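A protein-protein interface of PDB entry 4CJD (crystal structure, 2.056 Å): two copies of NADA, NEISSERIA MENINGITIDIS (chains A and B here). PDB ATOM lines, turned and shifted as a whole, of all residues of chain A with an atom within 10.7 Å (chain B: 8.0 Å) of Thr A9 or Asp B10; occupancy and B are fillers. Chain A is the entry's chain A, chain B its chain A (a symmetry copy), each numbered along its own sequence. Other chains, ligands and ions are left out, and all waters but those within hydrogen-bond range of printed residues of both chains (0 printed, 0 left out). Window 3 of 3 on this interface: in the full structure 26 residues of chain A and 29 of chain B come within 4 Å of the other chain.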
ATOM      1  N   PRO A   6      22.310   4.185   2.511  1.00  0.00           N
ATOM      2  CA  PRO A   6      22.725   5.486   1.978  1.00  0.00           C
ATOM      3  C   PRO A   6      24.237   5.593   1.802  1.00  0.00           C
ATOM      4  O   PRO A   6      24.980   4.761   2.334  1.00  0.00           O
ATOM      5  CB  PRO A   6      22.235   6.480   3.045  1.00  0.00           C
ATOM      6  CG  PRO A   6      22.025   5.663   4.273  1.00  0.00           C
ATOM      7  CD  PRO A   6      21.571   4.326   3.775  1.00  0.00           C
ATOM      8  N   PRO A   7      24.692   6.602   1.041  1.00  0.00           N
ATOM      9  CA  PRO A   7      26.114   6.946   1.089  1.00  0.00           C
ATOM     10  C   PRO A   7      26.395   7.781   2.332  1.00  0.00           C
ATOM     11  O   PRO A   7      25.680   8.746   2.595  1.00  0.00           O
ATOM     12  CB  PRO A   7      26.339   7.749  -0.202  1.00  0.00           C
ATOM     13  CG  PRO A   7      24.965   8.187  -0.654  1.00  0.00           C
ATOM     14  CD  PRO A   7      23.918   7.530   0.198  1.00  0.00           C
ATOM     15  N   SER A   8      27.395   7.382   3.108  1.00  0.00           N
ATOM     16  CA  SER A   8      27.844   8.162   4.258  1.00  0.00           C
ATOM     17  C   SER A   8      28.417   9.522   3.818  1.00  0.00           C
ATOM     18  O   SER A   8      28.767   9.709   2.648  1.00  0.00           O
ATOM     19  CB  SER A   8      28.905   7.385   5.032  1.00  0.00           C
ATOM     20  OG  SER A   8      30.085   7.271   4.243  1.00  0.00           O
ATOM     21  N   THR A   9      28.508  10.455   4.763  1.00  0.00           N
ATOM     22  CA  THR A   9      29.217  11.725   4.566  1.00  0.00           C
ATOM     23  C   THR A   9      30.621  11.498   4.036  1.00  0.00           C
ATOM     24  O   THR A   9      31.073  12.180   3.103  1.00  0.00           O
ATOM     25  CB  THR A   9      29.300  12.513   5.883  1.00  0.00           C
ATOM     26  OG1 THR A   9      27.973  12.786   6.343  1.00  0.00           O
ATOM     27  CG2 THR A   9      30.062  13.822   5.699  1.00  0.00           C
ATOM     28  N   ASP A  10      31.307  10.520   4.607  1.00  0.00           N
ATOM     29  CA  ASP A  10      32.651  10.187   4.162  1.00  0.00           C
ATOM     30  C   ASP A  10      32.689   9.786   2.684  1.00  0.00           C
ATOM     31  O   ASP A  10      33.547  10.256   1.955  1.00  0.00           O
ATOM     32  CB  ASP A  10      33.250   9.078   5.013  1.00  0.00           C
ATOM     33  CG  ASP A  10      34.729   8.863   4.721  1.00  0.00           C
ATOM     34  OD1 ASP A  10      35.530   9.793   4.981  1.00  0.00           O
ATOM     35  OD2 ASP A  10      35.092   7.762   4.248  1.00  0.00           O
ATOM     36  N   GLU A  11      31.763   8.937   2.240  1.00  0.00           N
ATOM     37  CA  GLU A  11      31.713   8.544   0.831  1.00  0.00           C
ATOM     38  C   GLU A  11      31.387   9.719  -0.086  1.00  0.00           C
ATOM     39  O   GLU A  11      31.960   9.846  -1.152  1.00  0.00           O
ATOM     40  CB  GLU A  11      30.682   7.437   0.600  1.00  0.00           C
ATOM     41  CG  GLU A  11      31.161   6.054   1.009  1.00  0.00           C
ATOM     42  CD  GLU A  11      30.054   5.008   0.945  1.00  0.00           C
ATOM     43  OE1 GLU A  11      28.981   5.224   1.558  1.00  0.00           O
ATOM     44  OE2 GLU A  11      30.259   3.975   0.269  1.00  0.00           O
ATOM     45  N   ILE A  12      30.444  10.559   0.330  1.00  0.00           N
ATOM     46  CA  ILE A  12      30.084  11.740  -0.455  1.00  0.00           C
ATOM     47  C   ILE A  12      31.299  12.632  -0.642  1.00  0.00           C
ATOM     48  O   ILE A  12      31.622  13.052  -1.763  1.00  0.00           O
ATOM     49  CB  ILE A  12      28.925  12.538   0.228  1.00  0.00           C
ATOM     50  CG1 ILE A  12      27.644  11.695   0.228  1.00  0.00           C
ATOM     51  CG2 ILE A  12      28.712  13.882  -0.479  1.00  0.00           C
ATOM     52  CD1 ILE A  12      26.450  12.297   1.012  1.00  0.00           C
ATOM     53  N   ALA A  13      31.984  12.910   0.462  1.00  0.00           N
ATOM     54  CA  ALA A  13      33.164  13.765   0.450  1.00  0.00           C
ATOM     55  C   ALA A  13      34.228  13.217  -0.499  1.00  0.00           C
ATOM     56  O   ALA A  13      34.836  13.963  -1.251  1.00  0.00           O
ATOM     57  CB  ALA A  13      33.726  13.910   1.854  1.00  0.00           C
ATOM     58  N   LYS A  14      34.447  11.903  -0.449  1.00  0.00           N
ATOM     59  CA  LYS A  14      35.489  11.273  -1.276  1.00  0.00           C
ATOM     60  C   LYS A  14      35.100  11.271  -2.736  1.00  0.00           C
ATOM     61  O   LYS A  14      35.932  11.463  -3.615  1.00  0.00           O
ATOM     62  CB  LYS A  14      35.760   9.846  -0.771  1.00  0.00           C
ATOM     63  CG  LYS A  14      36.558   9.847   0.532  1.00  0.00           C
ATOM     64  CD  LYS A  14      36.519   8.509   1.257  1.00  0.00           C
ATOM     65  CE  LYS A  14      37.711   8.384   2.195  1.00  0.00           C
ATOM     66  NZ  LYS A  14      37.531   7.231   3.150  1.00  0.00           N
ATOM     67  N   ALA A  15      33.812  11.082  -2.998  1.00  0.00           N
ATOM     68  CA  ALA A  15      33.335  11.115  -4.368  1.00  0.00           C
ATOM     69  C   ALA A  15      33.446  12.535  -4.924  1.00  0.00           C
ATOM     70  O   ALA A  15      33.763  12.737  -6.093  1.00  0.00           O
ATOM     71  CB  ALA A  15      31.884  10.605  -4.443  1.00  0.00           C
ATOM     72  N   ALA A  16      33.180  13.526  -4.081  1.00  0.00           N
ATOM     73  CA  ALA A  16      33.363  14.923  -4.499  1.00  0.00           C
ATOM     74  C   ALA A  16      34.843  15.221  -4.782  1.00  0.00           C
ATOM     75  O   ALA A  16      35.203  15.809  -5.810  1.00  0.00           O
ATOM     76  CB  ALA A  16      32.796  15.878  -3.417  1.00  0.00           C
ATOM     77  N   LEU A  17      35.720  14.786  -3.893  1.00  0.00           N
ATOM     78  CA  LEU A  17      37.146  15.036  -4.110  1.00  0.00           C
ATOM     79  C   LEU A  17      37.627  14.399  -5.408  1.00  0.00           C
ATOM     80  O   LEU A  17      38.289  15.054  -6.232  1.00  0.00           O
ATOM     81  CB  LEU A  17      37.969  14.532  -2.942  1.00  0.00           C
ATOM     82  CG  LEU A  17      39.385  15.105  -2.885  1.00  0.00           C
ATOM     83  CD1 LEU A  17      39.273  16.637  -2.786  1.00  0.00           C
ATOM     84  CD2 LEU A  17      40.092  14.498  -1.666  1.00  0.00           C
ATOM     85  N   ILE A  39      36.486   6.056  -8.077  1.00  0.00           N
ATOM     86  CA  ILE A  39      35.965   5.601  -6.814  1.00  0.00           C
ATOM     87  C   ILE A  39      35.702   4.115  -6.945  1.00  0.00           C
ATOM     88  O   ILE A  39      35.082   3.687  -7.921  1.00  0.00           O
ATOM     89  CB  ILE A  39      34.668   6.337  -6.451  1.00  0.00           C
ATOM     90  CG1 ILE A  39      34.958   7.776  -6.009  1.00  0.00           C
ATOM     91  CG2 ILE A  39      33.914   5.563  -5.381  1.00  0.00           C
ATOM     92  CD1 ILE A  39      35.449   7.878  -4.552  1.00  0.00           C
ATOM     93  N   GLY A  42      33.560   2.684  -2.729  1.00  0.00           N
ATOM     94  CA  GLY A  42      33.421   3.975  -2.074  1.00  0.00           C
ATOM     95  C   GLY A  42      34.724   4.635  -1.639  1.00  0.00           C
ATOM     96  O   GLY A  42      34.710   5.659  -0.921  1.00  0.00           O
ATOM     97  N   GLN A  43      35.854   4.051  -2.054  1.00  0.00           N
ATOM     98  CA  GLN A  43      37.162   4.633  -1.768  1.00  0.00           C
ATOM     99  C   GLN A  43      37.779   5.179  -3.061  1.00  0.00           C
ATOM    100  O   GLN A  43      37.594   4.607  -4.136  1.00  0.00           O
ATOM    101  CB  GLN A  43      38.101   3.604  -1.113  1.00  0.00           C
ATOM    102  CG  GLN A  43      37.642   3.085   0.269  1.00  0.00           C
ATOM    103  CD  GLN A  43      37.090   4.194   1.150  1.00  0.00           C
ATOM    104  OE1 GLN A  43      37.809   5.114   1.563  1.00  0.00           O
ATOM    105  NE2 GLN A  43      35.793   4.127   1.414  1.00  0.00           N
ATOM    106  N   PRO A  44      38.512   6.295  -2.962  1.00  0.00           N
ATOM    107  CA  PRO A  44      39.287   6.780  -4.112  1.00  0.00           C
ATOM    108  C   PRO A  44      40.430   5.824  -4.459  1.00  0.00           C
ATOM    109  O   PRO A  44      41.100   5.305  -3.570  1.00  0.00           O
ATOM    110  CB  PRO A  44      39.829   8.129  -3.634  1.00  0.00           C
ATOM    111  CG  PRO A  44      39.674   8.130  -2.163  1.00  0.00           C
ATOM    112  CD  PRO A  44      38.559   7.221  -1.820  1.00  0.00           C
ATOM    113  N   PRO B   7      28.084  25.441   8.798  1.00  0.00           N
ATOM    114  CA  PRO B   7      27.730  24.282   7.975  1.00  0.00           C
ATOM    115  C   PRO B   7      28.450  23.047   8.501  1.00  0.00           C
ATOM    116  O   PRO B   7      29.655  23.093   8.736  1.00  0.00           O
ATOM    117  CB  PRO B   7      28.218  24.671   6.569  1.00  0.00           C
ATOM    118  CG  PRO B   7      29.201  25.801   6.778  1.00  0.00           C
ATOM    119  CD  PRO B   7      29.185  26.228   8.216  1.00  0.00           C
ATOM    120  N   SER B   8      27.704  21.971   8.726  1.00  0.00           N
ATOM    121  CA  SER B   8      28.287  20.689   9.112  1.00  0.00           C
ATOM    122  C   SER B   8      29.180  20.125   7.991  1.00  0.00           C
ATOM    123  O   SER B   8      29.075  20.542   6.833  1.00  0.00           O
ATOM    124  CB  SER B   8      27.179  19.690   9.437  1.00  0.00           C
ATOM    125  OG  SER B   8      26.461  19.370   8.250  1.00  0.00           O
ATOM    126  N   THR B   9      30.045  19.179   8.350  1.00  0.00           N
ATOM    127  CA  THR B   9      30.817  18.393   7.379  1.00  0.00           C
ATOM    128  C   THR B   9      29.918  17.787   6.317  1.00  0.00           C
ATOM    129  O   THR B   9      30.225  17.829   5.115  1.00  0.00           O
ATOM    130  CB  THR B   9      31.592  17.268   8.082  1.00  0.00           C
ATOM    131  OG1 THR B   9      32.490  17.848   9.033  1.00  0.00           O
ATOM    132  CG2 THR B   9      32.375  16.425   7.081  1.00  0.00           C
ATOM    133  N   ASP B  10      28.790  17.247   6.751  1.00  0.00           N
ATOM    134  CA  ASP B  10      27.832  16.665   5.824  1.00  0.00           C
ATOM    135  C   ASP B  10      27.328  17.682   4.796  1.00  0.00           C
ATOM    136  O   ASP B  10      27.278  17.372   3.617  1.00  0.00           O
ATOM    137  CB  ASP B  10      26.653  16.053   6.566  1.00  0.00           C
ATOM    138  CG  ASP B  10      25.752  15.241   5.646  1.00  0.00           C
ATOM    139  OD1 ASP B  10      26.222  14.213   5.103  1.00  0.00           O
ATOM    140  OD2 ASP B  10      24.570  15.621   5.479  1.00  0.00           O
ATOM    141  N   GLU B  11      26.969  18.889   5.231  1.00  0.00           N
ATOM    142  CA  GLU B  11      26.518  19.924   4.300  1.00  0.00           C
ATOM    143  C   GLU B  11      27.622  20.360   3.341  1.00  0.00           C
ATOM    144  O   GLU B  11      27.373  20.572   2.169  1.00  0.00           O
ATOM    145  CB  GLU B  11      26.000  21.155   5.047  1.00  0.00           C
ATOM    146  CG  GLU B  11      24.596  20.991   5.605  1.00  0.00           C
ATOM    147  CD  GLU B  11      24.183  22.154   6.500  1.00  0.00           C
ATOM    148  OE1 GLU B  11      24.926  22.474   7.458  1.00  0.00           O
ATOM    149  OE2 GLU B  11      23.116  22.751   6.232  1.00  0.00           O
ATOM    150  N   ILE B  12      28.839  20.514   3.858  1.00  0.00           N
ATOM    151  CA  ILE B  12      29.974  20.890   3.018  1.00  0.00           C
ATOM    152  C   ILE B  12      30.181  19.853   1.926  1.00  0.00           C
ATOM    153  O   ILE B  12      30.300  20.187   0.737  1.00  0.00           O
ATOM    154  CB  ILE B  12      31.278  21.045   3.869  1.00  0.00           C
ATOM    155  CG1 ILE B  12      31.129  22.229   4.832  1.00  0.00           C
ATOM    156  CG2 ILE B  12      32.497  21.216   2.955  1.00  0.00           C
ATOM    157  CD1 ILE B  12      32.284  22.409   5.850  1.00  0.00           C
ATOM    158  N   ALA B  13      30.208  18.589   2.330  1.00  0.00           N
ATOM    159  CA  ALA B  13      30.412  17.480   1.405  1.00  0.00           C
ATOM    160  C   ALA B  13      29.350  17.480   0.308  1.00  0.00           C
ATOM    161  O   ALA B  13      29.658  17.276  -0.857  1.00  0.00           O
ATOM    162  CB  ALA B  13      30.406  16.159   2.154  1.00  0.00           C
ATOM    163  N   LYS B  14      28.095  17.704   0.697  1.00  0.00           N
ATOM    164  CA  LYS B  14      26.981  17.668  -0.266  1.00  0.00           C
ATOM    165  C   LYS B  14      27.028  18.857  -1.198  1.00  0.00           C
ATOM    166  O   LYS B  14      26.732  18.744  -2.382  1.00  0.00           O
ATOM    167  CB  LYS B  14      25.644  17.608   0.491  1.00  0.00           C
ATOM    168  CG  LYS B  14      25.393  16.226   1.089  1.00  0.00           C
ATOM    169  CD  LYS B  14      24.297  16.222   2.146  1.00  0.00           C
ATOM    170  CE  LYS B  14      23.718  14.823   2.301  1.00  0.00           C
ATOM    171  NZ  LYS B  14      22.872  14.720   3.544  1.00  0.00           N
ATOM    172  N   ALA B  15      27.436  20.002  -0.666  1.00  0.00           N
ATOM    173  CA  ALA B  15      27.562  21.187  -1.495  1.00  0.00           C
ATOM    174  C   ALA B  15      28.713  21.007  -2.487  1.00  0.00           C
ATOM    175  O   ALA B  15      28.638  21.442  -3.633  1.00  0.00           O
ATOM    176  CB  ALA B  15      27.780  22.435  -0.620  1.00  0.00           C
ATOM    177  N   ALA B  16      29.786  20.362  -2.043  1.00  0.00           N
ATOM    178  CA  ALA B  16      30.894  20.052  -2.957  1.00  0.00           C
ATOM    179  C   ALA B  16      30.444  19.072  -4.052  1.00  0.00           C
ATOM    180  O   ALA B  16      30.702  19.269  -5.246  1.00  0.00           O
ATOM    181  CB  ALA B  16      32.096  19.486  -2.158  1.00  0.00           C
ATOM    182  N   LEU B  17      29.734  18.026  -3.662  1.00  0.00           N
ATOM    183  CA  LEU B  17      29.273  17.061  -4.660  1.00  0.00           C
ATOM    184  C   LEU B  17      28.372  17.722  -5.695  1.00  0.00           C
ATOM    185  O   LEU B  17      28.568  17.555  -6.911  1.00  0.00           O
ATOM    186  CB  LEU B  17      28.553  15.902  -4.002  1.00  0.00           C
ATOM    187  CG  LEU B  17      28.406  14.671  -4.896  1.00  0.00           C
ATOM    188  CD1 LEU B  17      29.817  14.208  -5.301  1.00  0.00           C
ATOM    189  CD2 LEU B  17      27.653  13.596  -4.100  1.00  0.00           C
ATOM    190  N   ILE B  39      21.308  22.820  -4.232  1.00  0.00           N
ATOM    191  CA  ILE B  39      21.263  22.551  -2.817  1.00  0.00           C
ATOM    192  C   ILE B  39      20.064  23.289  -2.257  1.00  0.00           C
ATOM    193  O   ILE B  39      19.886  24.475  -2.543  1.00  0.00           O
ATOM    194  CB  ILE B  39      22.545  23.025  -2.121  1.00  0.00           C
ATOM    195  CG1 ILE B  39      23.719  22.091  -2.436  1.00  0.00           C
ATOM    196  CG2 ILE B  39      22.310  23.144  -0.623  1.00  0.00           C
ATOM    197  CD1 ILE B  39      23.712  20.801  -1.594  1.00  0.00           C
ATOM    198  N   GLY B  42      20.177  22.653   2.641  1.00  0.00           N
ATOM    199  CA  GLY B  42      21.437  21.941   2.767  1.00  0.00           C
ATOM    200  C   GLY B  42      21.454  20.528   2.195  1.00  0.00           C
ATOM    201  O   GLY B  42      22.428  19.769   2.399  1.00  0.00           O
ATOM    202  N   GLN B  43      20.377  20.158   1.491  1.00  0.00           N
ATOM    203  CA  GLN B  43      20.310  18.859   0.828  1.00  0.00           C
ATOM    204  C   GLN B  43      20.387  19.049  -0.692  1.00  0.00           C
ATOM    205  O   GLN B  43      19.873  20.031  -1.229  1.00  0.00           O
ATOM    206  CB  GLN B  43      19.026  18.102   1.213  1.00  0.00           C
ATOM    207  CG  GLN B  43      18.907  17.734   2.711  1.00  0.00           C
ATOM    208  CD  GLN B  43      20.220  17.235   3.291  1.00  0.00           C
ATOM    209  OE1 GLN B  43      20.734  16.172   2.914  1.00  0.00           O
ATOM    210  NE2 GLN B  43      20.786  18.022   4.194  1.00  0.00           N
ATOM    211  N   PRO B  44      21.040  18.112  -1.389  1.00  0.00           N
ATOM    212  CA  PRO B  44      21.004  18.118  -2.858  1.00  0.00           C
ATOM    213  C   PRO B  44      19.600  17.814  -3.384  1.00  0.00           C
ATOM    214  O   PRO B  44      18.912  16.944  -2.858  1.00  0.00           O
ATOM    215  CB  PRO B  44      21.985  17.008  -3.244  1.00  0.00           C
ATOM    216  CG  PRO B  44      22.190  16.205  -2.020  1.00  0.00           C
ATOM    217  CD  PRO B  44      21.938  17.077  -0.852  1.00  0.00           C
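Thr A9 touches just these residues of chain B: Thr B9 and Asp B10.
Asp B10 touches one residue of chain A.
No residue of chain B comes within 4 Å of Ser A8.
Ser B8 touches none of the printed residues of chain A.
Lys B14 touches just one residue of chain A: Ile A12 (3.9 Å).
Of the printed residues of chain A, Ala B13 touches Ile A12 and Ala A13.
Of the printed residues of chain B, Ile A12 touches Ala B13 (3.5 Å), Lys B14 (3.9 Å) and Leu B17 (3.8 Å).
The nearest residue of chain B that does not touch Thr A9 is Ala B13 (4.1 Å).
Thr B9 touches its own counterpart, Thr A9.
Ile A12 touches Ala B13, but with the chains exchanged Ala A13 does not touch Ile B12 (6.9 Å).
Ala B13 touches its own counterpart, Ala A13.
Ala A16 touches Leu B17, but with the chains exchanged Leu A17 does not touch Ala B16 (6.2 Å).
15 positions are printed for both chains.
Of the 8 pairs that touch across the chains among the printed residues, 3 have their exchanged pair printed and touching as well.
Hydrophobic or aromatic side chains of chain A that line the printed part of chain B: Ile A12 and Ala A16.
Among the printed residues, 8 pairs touch across the chains.
NZ of Lys B14 lies within hydrogen-bond range of OE1 of Gln B43 (2.7 Å).
The side-chain hydroxyl (OG) of Ser B8 lies close to the backbone NH (N) of Asp B10, 3.5 Å away.
NZ of Lys B14 lies within salt-bridge range of OD2 of Asp B10, 2.7 Å away.
The side-chain hydroxyl (OG1) of Thr A9 sits at hydrogen-bond distance from the side-chain carboxylate (OD1) of Asp B10 (2.6 Å).
Among the printed residues, merely in contact across the chains: Ile A12 with Ala B13, Ala A16 with Leu B17, Thr A9 with Thr B9, Ile A12 with Leu B17, Ala A16 with Ala B16, Ile A12 with Lys B14 and Ala A13 with Ala B13.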
